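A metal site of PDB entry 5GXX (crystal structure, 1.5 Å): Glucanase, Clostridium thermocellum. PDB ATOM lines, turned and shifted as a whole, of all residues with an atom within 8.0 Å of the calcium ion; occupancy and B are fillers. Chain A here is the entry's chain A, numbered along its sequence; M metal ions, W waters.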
ATOM      1  N   THR A 461     -23.141  35.935  -7.001  1.00  0.00           N
ATOM      2  CA  THR A 461     -22.098  34.913  -6.874  1.00  0.00           C
ATOM      3  C   THR A 461     -21.017  35.210  -7.905  1.00  0.00           C
ATOM      4  O   THR A 461     -21.342  35.456  -9.055  1.00  0.00           O
ATOM      5  CB  THR A 461     -22.690  33.523  -7.177  1.00  0.00           C
ATOM      6  OG1 THR A 461     -23.590  33.148  -6.129  1.00  0.00           O
ATOM      7  CG2 THR A 461     -21.588  32.454  -7.243  1.00  0.00           C
ATOM      8  N   TYR A 486     -24.902  25.751 -13.379  1.00  0.00           N
ATOM      9  CA  TYR A 486     -26.327  25.614 -13.139  1.00  0.00           C
ATOM     10  C   TYR A 486     -26.782  26.250 -11.836  1.00  0.00           C
ATOM     11  O   TYR A 486     -26.141  26.113 -10.795  1.00  0.00           O
ATOM     12  CB  TYR A 486     -26.721  24.125 -13.075  1.00  0.00           C
ATOM     13  CG  TYR A 486     -26.445  23.317 -14.319  1.00  0.00           C
ATOM     14  CD1 TYR A 486     -27.374  23.269 -15.357  1.00  0.00           C
ATOM     15  CD2 TYR A 486     -25.279  22.571 -14.424  1.00  0.00           C
ATOM     16  CE1 TYR A 486     -27.133  22.505 -16.493  1.00  0.00           C
ATOM     17  CE2 TYR A 486     -25.035  21.816 -15.555  1.00  0.00           C
ATOM     18  CZ  TYR A 486     -25.957  21.785 -16.585  1.00  0.00           C
ATOM     19  OH  TYR A 486     -25.705  21.018 -17.700  1.00  0.00           O
ATOM     20  N   MET A 487     -27.937  26.906 -11.917  1.00  0.00           N
ATOM     21  CA  MET A 487     -28.549  27.621 -10.801  1.00  0.00           C
ATOM     22  C   MET A 487     -30.012  27.248 -10.650  1.00  0.00           C
ATOM     23  O   MET A 487     -30.668  26.879 -11.626  1.00  0.00           O
ATOM     24  CB  MET A 487     -28.497  29.132 -11.077  1.00  0.00           C
ATOM     25  CG  MET A 487     -27.114  29.662 -11.345  1.00  0.00           C
ATOM     26  SD  MET A 487     -27.230  31.246 -12.197  1.00  0.00           S
ATOM     27  CE  MET A 487     -27.287  30.737 -13.917  1.00  0.00           C
ATOM     28  N   ASP A 488     -30.518  27.392  -9.432  1.00  0.00           N
ATOM     29  CA  ASP A 488     -31.946  27.322  -9.156  1.00  0.00           C
ATOM     30  C   ASP A 488     -32.407  28.757  -8.894  1.00  0.00           C
ATOM     31  O   ASP A 488     -31.919  29.406  -7.973  1.00  0.00           O
ATOM     32  CB  ASP A 488     -32.211  26.415  -7.946  1.00  0.00           C
ATOM     33  CG  ASP A 488     -33.682  26.206  -7.666  1.00  0.00           C
ATOM     34  OD1 ASP A 488     -34.508  27.051  -8.058  1.00  0.00           O
ATOM     35  OD2 ASP A 488     -34.033  25.167  -7.063  1.00  0.00           O
ATOM     36  N   LEU A 489     -33.308  29.240  -9.742  1.00  0.00           N
ATOM     37  CA  LEU A 489     -33.765  30.627  -9.650  1.00  0.00           C
ATOM     38  C   LEU A 489     -35.124  30.767  -8.965  1.00  0.00           C
ATOM     39  O   LEU A 489     -35.786  31.788  -9.099  1.00  0.00           O
ATOM     40  CB  LEU A 489     -33.794  31.276 -11.042  1.00  0.00           C
ATOM     41  CG  LEU A 489     -32.444  31.390 -11.784  1.00  0.00           C
ATOM     42  CD1 LEU A 489     -32.643  32.219 -13.050  1.00  0.00           C
ATOM     43  CD2 LEU A 489     -31.336  31.977 -10.933  1.00  0.00           C
ATOM     44  N   THR A 490     -35.511  29.744  -8.197  1.00  0.00           N
ATOM     45  CA  THR A 490     -36.768  29.761  -7.460  1.00  0.00           C
ATOM     46  C   THR A 490     -36.922  31.025  -6.602  1.00  0.00           C
ATOM     47  O   THR A 490     -37.978  31.647  -6.617  1.00  0.00           O
ATOM     48  CB  THR A 490     -36.965  28.519  -6.557  1.00  0.00           C
ATOM     49  OG1 THR A 490     -37.024  27.353  -7.378  1.00  0.00           O
ATOM     50  CG2 THR A 490     -38.275  28.603  -5.772  1.00  0.00           C
ATOM     51  N   GLU A 491     -35.873  31.369  -5.856  1.00  0.00           N
ATOM     52  CA  GLU A 491     -35.908  32.516  -4.946  1.00  0.00           C
ATOM     53  C   GLU A 491     -35.995  33.868  -5.658  1.00  0.00           C
ATOM     54  O   GLU A 491     -36.434  34.859  -5.079  1.00  0.00           O
ATOM     55  CB  GLU A 491     -34.702  32.499  -3.992  1.00  0.00           C
ATOM     56  CG  GLU A 491     -33.376  32.928  -4.612  1.00  0.00           C
ATOM     57  CD  GLU A 491     -32.624  31.801  -5.303  1.00  0.00           C
ATOM     58  OE1 GLU A 491     -33.110  30.658  -5.326  1.00  0.00           O
ATOM     59  OE2 GLU A 491     -31.517  32.083  -5.813  1.00  0.00           O
ATOM     60  N   VAL A 492     -35.580  33.887  -6.923  1.00  0.00           N
ATOM     61  CA  VAL A 492     -35.645  35.088  -7.752  1.00  0.00           C
ATOM     62  C   VAL A 492     -37.103  35.363  -8.070  1.00  0.00           C
ATOM     63  O   VAL A 492     -37.609  36.464  -7.859  1.00  0.00           O
ATOM     64  CB  VAL A 492     -34.827  34.920  -9.045  1.00  0.00           C
ATOM     65  CG1 VAL A 492     -34.982  36.128  -9.963  1.00  0.00           C
ATOM     66  CG2 VAL A 492     -33.371  34.667  -8.723  1.00  0.00           C
ATOM     67  N   ASN A 526     -37.382  25.455 -12.375  1.00  0.00           N
ATOM     68  CA  ASN A 526     -36.673  26.697 -12.053  1.00  0.00           C
ATOM     69  C   ASN A 526     -35.163  26.609 -12.238  1.00  0.00           C
ATOM     70  O   ASN A 526     -34.422  27.451 -11.721  1.00  0.00           O
ATOM     71  CB  ASN A 526     -37.036  27.178 -10.650  1.00  0.00           C
ATOM     72  CG  ASN A 526     -38.482  27.632 -10.521  1.00  0.00           C
ATOM     73  OD1 ASN A 526     -39.148  27.940 -11.507  1.00  0.00           O
ATOM     74  ND2 ASN A 526     -38.967  27.687  -9.281  1.00  0.00           N
ATOM     75  N   PHE A 564     -32.442  38.707  -1.927  1.00  0.00           N
ATOM     76  CA  PHE A 564     -32.988  37.377  -2.195  1.00  0.00           C
ATOM     77  C   PHE A 564     -32.008  36.332  -2.725  1.00  0.00           C
ATOM     78  O   PHE A 564     -32.263  35.140  -2.561  1.00  0.00           O
ATOM     79  CB  PHE A 564     -34.210  37.441  -3.113  1.00  0.00           C
ATOM     80  CG  PHE A 564     -33.930  38.008  -4.481  1.00  0.00           C
ATOM     81  CD1 PHE A 564     -33.333  37.225  -5.470  1.00  0.00           C
ATOM     82  CD2 PHE A 564     -34.268  39.317  -4.784  1.00  0.00           C
ATOM     83  CE1 PHE A 564     -33.084  37.756  -6.716  1.00  0.00           C
ATOM     84  CE2 PHE A 564     -34.043  39.848  -6.036  1.00  0.00           C
ATOM     85  CZ  PHE A 564     -33.438  39.060  -7.020  1.00  0.00           C
ATOM     86  N   TRP A 565     -30.919  36.768  -3.369  1.00  0.00           N
ATOM     87  CA  TRP A 565     -30.033  35.837  -4.085  1.00  0.00           C
ATOM     88  C   TRP A 565     -29.598  34.701  -3.171  1.00  0.00           C
ATOM     89  O   TRP A 565     -29.095  34.945  -2.081  1.00  0.00           O
ATOM     90  CB  TRP A 565     -28.816  36.605  -4.616  1.00  0.00           C
ATOM     91  CG  TRP A 565     -27.920  35.761  -5.497  1.00  0.00           C
ATOM     92  CD1 TRP A 565     -26.669  35.312  -5.189  1.00  0.00           C
ATOM     93  CD2 TRP A 565     -28.198  35.307  -6.815  1.00  0.00           C
ATOM     94  NE1 TRP A 565     -26.158  34.582  -6.243  1.00  0.00           N
ATOM     95  CE2 TRP A 565     -27.079  34.566  -7.257  1.00  0.00           C
ATOM     96  CE3 TRP A 565     -29.307  35.430  -7.676  1.00  0.00           C
ATOM     97  CZ2 TRP A 565     -27.027  33.956  -8.514  1.00  0.00           C
ATOM     98  CZ3 TRP A 565     -29.242  34.838  -8.932  1.00  0.00           C
ATOM     99  CH2 TRP A 565     -28.121  34.099  -9.333  1.00  0.00           C
ATOM    100  N   ASP A 566     -29.797  33.466  -3.617  1.00  0.00           N
ATOM    101  CA  ASP A 566     -29.459  32.304  -2.793  1.00  0.00           C
ATOM    102  C   ASP A 566     -28.664  31.269  -3.610  1.00  0.00           C
ATOM    103  O   ASP A 566     -29.250  30.483  -4.341  1.00  0.00           O
ATOM    104  CB  ASP A 566     -30.726  31.686  -2.192  1.00  0.00           C
ATOM    105  CG  ASP A 566     -30.421  30.518  -1.255  1.00  0.00           C
ATOM    106  OD1 ASP A 566     -29.265  30.345  -0.837  1.00  0.00           O
ATOM    107  OD2 ASP A 566     -31.374  29.782  -0.924  1.00  0.00           O
ATOM    108  N   PRO A 567     -27.331  31.305  -3.497  1.00  0.00           N
ATOM    109  CA  PRO A 567     -26.526  30.326  -4.245  1.00  0.00           C
ATOM    110  C   PRO A 567     -26.588  28.924  -3.652  1.00  0.00           C
ATOM    111  O   PRO A 567     -26.233  27.964  -4.351  1.00  0.00           O
ATOM    112  CB  PRO A 567     -25.118  30.882  -4.123  1.00  0.00           C
ATOM    113  CG  PRO A 567     -25.116  31.600  -2.793  1.00  0.00           C
ATOM    114  CD  PRO A 567     -26.480  32.225  -2.719  1.00  0.00           C
ATOM    115  N   THR A 568     -27.018  28.797  -2.395  1.00  0.00           N
ATOM    116  CA  THR A 568     -27.010  27.524  -1.662  1.00  0.00           C
ATOM    117  C   THR A 568     -27.967  26.466  -2.218  1.00  0.00           C
ATOM    118  O   THR A 568     -27.890  25.302  -1.814  1.00  0.00           O
ATOM    119  CB  THR A 568     -27.234  27.712  -0.126  1.00  0.00           C
ATOM    120  OG1 THR A 568     -28.623  27.942   0.152  1.00  0.00           O
ATOM    121  CG2 THR A 568     -26.392  28.845   0.436  1.00  0.00           C
ATOM    122  N   ASN A 569     -28.836  26.839  -3.153  1.00  0.00           N
ATOM    123  CA  ASN A 569     -29.667  25.839  -3.831  1.00  0.00           C
ATOM    124  C   ASN A 569     -29.290  25.656  -5.303  1.00  0.00           C
ATOM    125  O   ASN A 569     -30.031  25.044  -6.076  1.00  0.00           O
ATOM    126  CB  ASN A 569     -31.174  26.112  -3.645  1.00  0.00           C
ATOM    127  CG  ASN A 569     -31.642  27.416  -4.296  1.00  0.00           C
ATOM    128  OD1 ASN A 569     -30.933  28.027  -5.098  1.00  0.00           O
ATOM    129  ND2 ASN A 569     -32.856  27.836  -3.940  1.00  0.00           N
ATOM    130  N   ASP A 570     -28.141  26.214  -5.688  1.00  0.00           N
ATOM    131  CA  ASP A 570     -27.672  26.151  -7.068  1.00  0.00           C
ATOM    132  C   ASP A 570     -26.808  24.909  -7.270  1.00  0.00           C
ATOM    133  O   ASP A 570     -25.885  24.659  -6.485  1.00  0.00           O
ATOM    134  CB  ASP A 570     -26.863  27.397  -7.416  1.00  0.00           C
ATOM    135  CG  ASP A 570     -27.716  28.666  -7.402  1.00  0.00           C
ATOM    136  OD1 ASP A 570     -28.954  28.609  -7.183  1.00  0.00           O
ATOM    137  OD2 ASP A 570     -27.101  29.738  -7.626  1.00  0.00           O
ATOM    138  N   PHE A 571     -27.146  24.125  -8.296  1.00  0.00           N
ATOM    139  CA  PHE A 571     -26.484  22.841  -8.568  1.00  0.00           C
ATOM    140  C   PHE A 571     -24.958  22.983  -8.656  1.00  0.00           C
ATOM    141  O   PHE A 571     -24.219  22.183  -8.093  1.00  0.00           O
ATOM    142  CB  PHE A 571     -27.050  22.217  -9.844  1.00  0.00           C
ATOM    143  CG  PHE A 571     -26.388  20.915 -10.246  1.00  0.00           C
ATOM    144  CD1 PHE A 571     -25.269  20.905 -11.058  1.00  0.00           C
ATOM    145  CD2 PHE A 571     -26.919  19.698  -9.812  1.00  0.00           C
ATOM    146  CE1 PHE A 571     -24.676  19.700 -11.440  1.00  0.00           C
ATOM    147  CE2 PHE A 571     -26.331  18.492 -10.186  1.00  0.00           C
ATOM    148  CZ  PHE A 571     -25.209  18.490 -10.994  1.00  0.00           C
ATOM    149  N   TYR A 573     -22.977  25.331  -7.397  1.00  0.00           N
ATOM    150  CA  TYR A 573     -22.345  25.884  -6.199  1.00  0.00           C
ATOM    151  C   TYR A 573     -21.971  24.813  -5.179  1.00  0.00           C
ATOM    152  O   TYR A 573     -21.178  25.083  -4.272  1.00  0.00           O
ATOM    153  CB  TYR A 573     -23.323  26.866  -5.541  1.00  0.00           C
ATOM    154  CG  TYR A 573     -22.702  27.982  -4.744  1.00  0.00           C
ATOM    155  CD1 TYR A 573     -21.946  28.983  -5.369  1.00  0.00           C
ATOM    156  CD2 TYR A 573     -22.912  28.089  -3.365  1.00  0.00           C
ATOM    157  CE1 TYR A 573     -21.425  30.037  -4.633  1.00  0.00           C
ATOM    158  CE2 TYR A 573     -22.386  29.144  -2.637  1.00  0.00           C
ATOM    159  CZ  TYR A 573     -21.645  30.118  -3.266  1.00  0.00           C
ATOM    160  OH  TYR A 573     -21.127  31.163  -2.534  1.00  0.00           O
HETATM  161 CA    CA M   1     -30.538  30.027  -6.219  1.00  0.00          CA
HETATM  162  O   HOH W   1     -29.184  31.543  -7.458  1.00  0.00           O
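OG1 of Thr 490 sits at hydrogen-bond distance from OD1 of Asp 488 (2.6 Å).
OD1 of Asp 566 is in hydrogen-bond range of OG1 of Thr 568, 2.7 Å away.
Of the 18 residues printed, 5 come within 4 Å of the calcium ion.
The nearest printed residue that does not touch the calcium ion is Pro 567 (4.4 Å).
The calcium ion is bound by the side-chain carboxylate (OE2) of Glu 491, the backbone carbonyl oxygen (O) of Asp 488, the backbone carbonyl oxygen (O) of Asp 566, the side-chain amide oxygen (OD1) of Asn 569, the side-chain carboxylate (OD1) of Asp 570, water W1 and the side-chain carboxylate (OE1) of Glu 491.
The calcium ion has seven donor atoms within binding distance.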
